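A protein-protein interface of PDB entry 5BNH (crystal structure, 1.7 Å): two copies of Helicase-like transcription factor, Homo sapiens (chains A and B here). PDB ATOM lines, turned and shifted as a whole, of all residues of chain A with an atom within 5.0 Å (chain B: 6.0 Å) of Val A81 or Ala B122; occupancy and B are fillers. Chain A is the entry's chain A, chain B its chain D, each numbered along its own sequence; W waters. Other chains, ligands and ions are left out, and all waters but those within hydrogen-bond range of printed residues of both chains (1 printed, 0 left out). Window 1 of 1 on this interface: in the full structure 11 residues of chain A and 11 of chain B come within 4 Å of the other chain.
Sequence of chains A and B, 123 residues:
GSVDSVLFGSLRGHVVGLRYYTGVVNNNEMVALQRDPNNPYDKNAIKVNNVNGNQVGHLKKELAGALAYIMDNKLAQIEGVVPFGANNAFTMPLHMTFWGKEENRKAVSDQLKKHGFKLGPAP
The side-chain amide nitrogen (ND2) of Asn A28 is in hydrogen-bond range of the backbone carbonyl oxygen (O) of Phe B8. The side-chain amide oxygen of Asn A28 is in hydrogen-bond range of the backbone NH of Ala B122 (2.8 Å).
OD1 of Asn A28 touches CA of Pro B121, 3.4 Å away. CG of Met A30 touches CD1 of Leu B7 (3.8 Å). Val A81 touches Leu B7. CG1 of Val A81 touches O of Ala B122 (3.5 Å). Pro A83 touches Pro B121. His A95 touches Pro B123.
Of the 10 printed residues of chain B, 5 touch a printed residue of chain A. Hydrophobic or aromatic side chains of chain B within 4 Å of the printed part of chain A: Leu B7, Pro B121, Ala B122 and Pro B123. Of the 12 printed residues of chain A, 5 touch a printed residue of chain B. Among the printed residues, 8 pairs touch across the chains.
No position is printed for both chains. Of the 8 pairs that touch across the chains among the printed residues, none has its exchanged pair printed and touching as well.
The backbone NH (N) of Phe B8 lies within hydrogen-bond range of the backbone carbonyl oxygen (O) of Phe B98 (2.8 Å). The backbone carbonyl oxygen (O) of His A95 sits at hydrogen-bond distance from the backbone NH (N) of Val A81 (2.8 Å). The side-chain hydroxyl (OG) of Ser B10 is in hydrogen-bond range of the backbone carbonyl oxygen (O) of Pro B121 (2.8 Å). The chain-end carboxylate of Pro B123 is in hydrogen-bond range of the side-chain hydroxyl of Thr B97, 2.6 Å away. The backbone NH (N) of Asn A28 sits at hydrogen-bond distance from the backbone carbonyl oxygen (O) of Val A82, 2.8 Å away.
Water W1 bridges O of Pro B123 and NE2 of His A95.
Of the printed residues of chain B, Met A30 touches Leu B7. Val A31 touches none of the printed residues of chain B. Glu A79 touches none of the printed residues of chain B. Of the printed residues of chain B, Pro A83 touches Pro B121 (3.5 Å). Of the printed residues of chain B, His A95 touches Pro B123. Printed residues of chain A within 4 Å of Leu B7: Met A30 and Val A81. Of the printed residues of chain A, Phe B8 touches Asn A28. The nearest residue of chain A that does not touch Ala B122 is Pro A83 (4.3 Å). The nearest printed residue of chain B that does not touch Pro A83 is Ala B122 (4.3 Å).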
ATOM      1  N   ASN A  28      13.574 -27.188  10.023  1.00  0.00           N
ATOM      2  CA  ASN A  28      14.647 -26.448   9.459  1.00  0.00           C
ATOM      3  C   ASN A  28      14.361 -25.669   8.212  1.00  0.00           C
ATOM      4  O   ASN A  28      15.181 -25.775   7.248  1.00  0.00           O
ATOM      5  CB  ASN A  28      15.818 -27.431   9.189  1.00  0.00           C
ATOM      6  CG  ASN A  28      17.107 -26.701   8.879  1.00  0.00           C
ATOM      7  OD1 ASN A  28      17.362 -25.641   9.453  1.00  0.00           O
ATOM      8  ND2 ASN A  28      17.950 -27.329   8.072  1.00  0.00           N
ATOM      9  N   GLU A  29      13.241 -24.905   8.201  1.00  0.00           N
ATOM     10  CA  GLU A  29      12.646 -24.278   7.063  1.00  0.00           C
ATOM     11  C   GLU A  29      12.226 -22.806   7.345  1.00  0.00           C
ATOM     12  O   GLU A  29      11.830 -22.477   8.491  1.00  0.00           O
ATOM     13  CB  GLU A  29      11.393 -25.085   6.706  1.00  0.00           C
ATOM     14  CG  GLU A  29      10.626 -24.563   5.510  1.00  0.00           C
ATOM     15  CD  GLU A  29       9.592 -25.557   4.880  1.00  0.00           C
ATOM     16  OE1 GLU A  29       8.406 -25.520   5.350  1.00  0.00           O
ATOM     17  OE2 GLU A  29       9.984 -26.305   3.862  1.00  0.00           O
ATOM     18  N   MET A  30      12.328 -21.932   6.350  1.00  0.00           N
ATOM     19  CA  MET A  30      11.858 -20.565   6.458  1.00  0.00           C
ATOM     20  C   MET A  30      10.351 -20.477   6.642  1.00  0.00           C
ATOM     21  O   MET A  30       9.599 -21.375   6.138  1.00  0.00           O
ATOM     22  CB  MET A  30      12.228 -19.709   5.271  1.00  0.00           C
ATOM     23  CG  MET A  30      13.725 -19.416   5.161  1.00  0.00           C
ATOM     24  SD  MET A  30      14.191 -18.165   3.932  1.00  0.00           S
ATOM     25  CE  MET A  30      13.212 -16.766   4.480  1.00  0.00           C
ATOM     26  N   VAL A  31       9.941 -19.440   7.398  1.00  0.00           N
ATOM     27  CA  VAL A  31       8.533 -19.059   7.499  1.00  0.00           C
ATOM     28  C   VAL A  31       8.353 -17.580   7.218  1.00  0.00           C
ATOM     29  O   VAL A  31       9.336 -16.866   7.160  1.00  0.00           O
ATOM     30  CB  VAL A  31       7.963 -19.434   8.869  1.00  0.00           C
ATOM     31  CG1 VAL A  31       7.916 -20.932   9.022  1.00  0.00           C
ATOM     32  CG2 VAL A  31       8.760 -18.800  10.007  1.00  0.00           C
ATOM     33  N   GLU A  79      13.629 -12.118   9.660  1.00  0.00           N
ATOM     34  CA  GLU A  79      13.518 -13.408   8.935  1.00  0.00           C
ATOM     35  C   GLU A  79      13.367 -14.524   9.930  1.00  0.00           C
ATOM     36  O   GLU A  79      14.175 -14.657  10.820  1.00  0.00           O
ATOM     37  CB  GLU A  79      14.747 -13.684   8.079  1.00  0.00           C
ATOM     38  CG  GLU A  79      14.905 -12.671   6.925  1.00  0.00           C
ATOM     39  CD  GLU A  79      13.744 -12.688   5.928  1.00  0.00           C
ATOM     40  OE1 GLU A  79      13.329 -13.802   5.514  1.00  0.00           O
ATOM     41  OE2 GLU A  79      13.225 -11.597   5.558  1.00  0.00           O
ATOM     42  N   GLY A  80      12.422 -15.429   9.646  1.00  0.00           N
ATOM     43  CA  GLY A  80      12.088 -16.478  10.580  1.00  0.00           C
ATOM     44  C   GLY A  80      12.482 -17.827  10.026  1.00  0.00           C
ATOM     45  O   GLY A  80      12.223 -18.069   8.838  1.00  0.00           O
ATOM     46  N   VAL A  81      13.068 -18.704  10.851  1.00  0.00           N
ATOM     47  CA  VAL A  81      13.274 -20.102  10.488  1.00  0.00           C
ATOM     48  C   VAL A  81      12.814 -20.939  11.616  1.00  0.00           C
ATOM     49  O   VAL A  81      13.031 -20.560  12.779  1.00  0.00           O
ATOM     50  CB  VAL A  81      14.794 -20.336  10.232  1.00  0.00           C
ATOM     51  CG1 VAL A  81      15.119 -21.806  10.100  1.00  0.00           C
ATOM     52  CG2 VAL A  81      15.229 -19.466   9.086  1.00  0.00           C
ATOM     53  N   VAL A  82      12.161 -22.090  11.346  1.00  0.00           N
ATOM     54  CA  VAL A  82      11.837 -23.043  12.362  1.00  0.00           C
ATOM     55  C   VAL A  82      12.957 -24.079  12.389  1.00  0.00           C
ATOM     56  O   VAL A  82      13.130 -24.836  11.428  1.00  0.00           O
ATOM     57  CB  VAL A  82      10.481 -23.695  12.084  1.00  0.00           C
ATOM     58  CG1 VAL A  82      10.249 -24.804  13.060  1.00  0.00           C
ATOM     59  CG2 VAL A  82       9.369 -22.665  12.200  1.00  0.00           C
ATOM     60  N   PRO A  83      13.780 -24.063  13.454  1.00  0.00           N
ATOM     61  CA  PRO A  83      14.999 -24.846  13.451  1.00  0.00           C
ATOM     62  C   PRO A  83      14.776 -26.329  13.734  1.00  0.00           C
ATOM     63  O   PRO A  83      15.516 -27.197  13.184  1.00  0.00           O
ATOM     64  CB  PRO A  83      15.841 -24.188  14.553  1.00  0.00           C
ATOM     65  CG  PRO A  83      14.795 -23.634  15.489  1.00  0.00           C
ATOM     66  CD  PRO A  83      13.643 -23.210  14.658  1.00  0.00           C
ATOM     67  N   PRO A  93       9.426 -23.921  18.114  1.00  0.00           N
ATOM     68  CA  PRO A  93      10.531 -23.010  18.084  1.00  0.00           C
ATOM     69  C   PRO A  93      10.626 -22.133  16.880  1.00  0.00           C
ATOM     70  O   PRO A  93      10.353 -22.579  15.778  1.00  0.00           O
ATOM     71  CB  PRO A  93      11.775 -23.949  18.162  1.00  0.00           C
ATOM     72  CG  PRO A  93      11.277 -25.205  18.713  1.00  0.00           C
ATOM     73  CD  PRO A  93       9.839 -25.316  18.308  1.00  0.00           C
ATOM     74  N   LEU A  94      11.044 -20.904  17.073  1.00  0.00           N
ATOM     75  CA  LEU A  94      11.281 -20.005  15.973  1.00  0.00           C
ATOM     76  C   LEU A  94      12.559 -19.204  16.212  1.00  0.00           C
ATOM     77  O   LEU A  94      12.733 -18.627  17.304  1.00  0.00           O
ATOM     78  CB  LEU A  94      10.108 -19.045  15.860  1.00  0.00           C
ATOM     79  CG  LEU A  94      10.166 -18.080  14.703  1.00  0.00           C
ATOM     80  CD1 LEU A  94      10.066 -18.714  13.348  1.00  0.00           C
ATOM     81  CD2 LEU A  94       9.136 -16.991  14.906  1.00  0.00           C
ATOM     82  N   HIS A  95      13.442 -19.188  15.199  1.00  0.00           N
ATOM     83  CA  HIS A  95      14.580 -18.341  15.237  1.00  0.00           C
ATOM     84  C   HIS A  95      14.385 -17.163  14.320  1.00  0.00           C
ATOM     85  O   HIS A  95      14.044 -17.351  13.098  1.00  0.00           O
ATOM     86  CB  HIS A  95      15.798 -19.185  14.720  1.00  0.00           C
ATOM     87  CG  HIS A  95      17.099 -18.485  14.795  1.00  0.00           C
ATOM     88  ND1 HIS A  95      17.427 -17.365  14.042  1.00  0.00           N
ATOM     89  CD2 HIS A  95      18.162 -18.734  15.563  1.00  0.00           C
ATOM     90  CE1 HIS A  95      18.650 -16.969  14.357  1.00  0.00           C
ATOM     91  NE2 HIS A  95      19.126 -17.806  15.250  1.00  0.00           N
ATOM     92  N   LEU B   7      17.857 -22.842   2.586  1.00  0.00           N
ATOM     93  CA  LEU B   7      18.884 -22.997   3.704  1.00  0.00           C
ATOM     94  C   LEU B   7      19.106 -24.465   3.944  1.00  0.00           C
ATOM     95  O   LEU B   7      18.149 -25.246   4.049  1.00  0.00           O
ATOM     96  CB  LEU B   7      18.295 -22.384   5.008  1.00  0.00           C
ATOM     97  CG  LEU B   7      18.088 -20.897   4.869  1.00  0.00           C
ATOM     98  CD1 LEU B   7      17.270 -20.414   6.081  1.00  0.00           C
ATOM     99  CD2 LEU B   7      19.437 -20.222   4.850  1.00  0.00           C
ATOM    100  N   PHE B   8      20.357 -24.902   4.032  1.00  0.00           N
ATOM    101  CA  PHE B   8      20.686 -26.272   4.359  1.00  0.00           C
ATOM    102  C   PHE B   8      20.869 -26.418   5.853  1.00  0.00           C
ATOM    103  O   PHE B   8      20.618 -27.482   6.433  1.00  0.00           O
ATOM    104  CB  PHE B   8      21.985 -26.754   3.703  1.00  0.00           C
ATOM    105  CG  PHE B   8      21.937 -26.958   2.189  1.00  0.00           C
ATOM    106  CD1 PHE B   8      20.748 -27.027   1.489  1.00  0.00           C
ATOM    107  CD2 PHE B   8      23.107 -27.080   1.497  1.00  0.00           C
ATOM    108  CE1 PHE B   8      20.737 -27.272   0.114  1.00  0.00           C
ATOM    109  CE2 PHE B   8      23.135 -27.278   0.139  1.00  0.00           C
ATOM    110  CZ  PHE B   8      21.924 -27.368  -0.555  1.00  0.00           C
ATOM    111  N   GLY B   9      21.504 -25.418   6.461  1.00  0.00           N
ATOM    112  CA  GLY B   9      21.892 -25.630   7.885  1.00  0.00           C
ATOM    113  C   GLY B   9      23.015 -24.719   8.218  1.00  0.00           C
ATOM    114  O   GLY B   9      23.333 -23.809   7.468  1.00  0.00           O
ATOM    115  N   SER B  10      23.641 -24.967   9.384  1.00  0.00           N
ATOM    116  CA  SER B  10      24.770 -24.126   9.784  1.00  0.00           C
ATOM    117  C   SER B  10      25.862 -24.922  10.435  1.00  0.00           C
ATOM    118  O   SER B  10      25.646 -26.074  10.888  1.00  0.00           O
ATOM    119  CB  SER B  10      24.293 -23.115  10.796  1.00  0.00           C
ATOM    120  OG  SER B  10      23.846 -23.731  11.979  1.00  0.00           O
ATOM    121  N   THR B  97      26.502 -20.127   7.610  1.00  0.00           N
ATOM    122  CA  THR B  97      25.212 -20.557   7.076  1.00  0.00           C
ATOM    123  C   THR B  97      25.401 -21.128   5.678  1.00  0.00           C
ATOM    124  O   THR B  97      26.080 -20.541   4.844  1.00  0.00           O
ATOM    125  CB  THR B  97      24.280 -19.342   6.961  1.00  0.00           C
ATOM    126  OG1 THR B  97      24.140 -18.701   8.243  1.00  0.00           O
ATOM    127  CG2 THR B  97      23.003 -19.776   6.472  1.00  0.00           C
ATOM    128  N   PHE B  98      24.779 -22.273   5.430  1.00  0.00           N
ATOM    129  CA  PHE B  98      24.914 -23.001   4.184  1.00  0.00           C
ATOM    130  C   PHE B  98      23.595 -22.972   3.467  1.00  0.00           C
ATOM    131  O   PHE B  98      22.558 -23.203   4.064  1.00  0.00           O
ATOM    132  CB  PHE B  98      25.252 -24.472   4.406  1.00  0.00           C
ATOM    133  CG  PHE B  98      26.635 -24.754   4.922  1.00  0.00           C
ATOM    134  CD1 PHE B  98      27.508 -25.528   4.147  1.00  0.00           C
ATOM    135  CD2 PHE B  98      27.112 -24.278   6.153  1.00  0.00           C
ATOM    136  CE1 PHE B  98      28.766 -25.872   4.562  1.00  0.00           C
ATOM    137  CE2 PHE B  98      28.417 -24.590   6.544  1.00  0.00           C
ATOM    138  CZ  PHE B  98      29.253 -25.366   5.747  1.00  0.00           C
ATOM    139  N   GLY B 120      24.028 -28.160  11.705  1.00  0.00           N
ATOM    140  CA  GLY B 120      22.962 -27.838  12.655  1.00  0.00           C
ATOM    141  C   GLY B 120      21.897 -27.113  11.881  1.00  0.00           C
ATOM    142  O   GLY B 120      21.996 -26.893  10.695  1.00  0.00           O
ATOM    143  N   PRO B 121      20.803 -26.774  12.553  1.00  0.00           N
ATOM    144  CA  PRO B 121      19.751 -25.995  11.908  1.00  0.00           C
ATOM    145  C   PRO B 121      20.198 -24.648  11.416  1.00  0.00           C
ATOM    146  O   PRO B 121      21.111 -24.068  11.921  1.00  0.00           O
ATOM    147  CB  PRO B 121      18.719 -25.806  12.969  1.00  0.00           C
ATOM    148  CG  PRO B 121      19.187 -26.436  14.177  1.00  0.00           C
ATOM    149  CD  PRO B 121      20.516 -27.110  13.934  1.00  0.00           C
ATOM    150  N   ALA B 122      19.506 -24.171  10.396  1.00  0.00           N
ATOM    151  CA  ALA B 122      19.721 -22.853   9.886  1.00  0.00           C
ATOM    152  C   ALA B 122      19.089 -21.798  10.808  1.00  0.00           C
ATOM    153  O   ALA B 122      18.233 -22.144  11.626  1.00  0.00           O
ATOM    154  CB  ALA B 122      19.072 -22.763   8.510  1.00  0.00           C
ATOM    155  N   PRO B 123      19.467 -20.533  10.675  1.00  0.00           N
ATOM    156  CA  PRO B 123      20.587 -20.056   9.876  1.00  0.00           C
ATOM    157  C   PRO B 123      21.877 -20.287  10.682  1.00  0.00           C
ATOM    158  O   PRO B 123      21.900 -20.656  11.891  1.00  0.00           O
ATOM    159  CB  PRO B 123      20.326 -18.521   9.807  1.00  0.00           C
ATOM    160  CG  PRO B 123      19.717 -18.231  11.091  1.00  0.00           C
ATOM    161  CD  PRO B 123      18.832 -19.425  11.416  1.00  0.00           C
ATOM    162  OXT PRO B 123      22.918 -20.070  10.062  1.00  0.00           O
HETATM  163  O   HOH W   1      22.333 -18.824  14.641  1.00  0.00           O
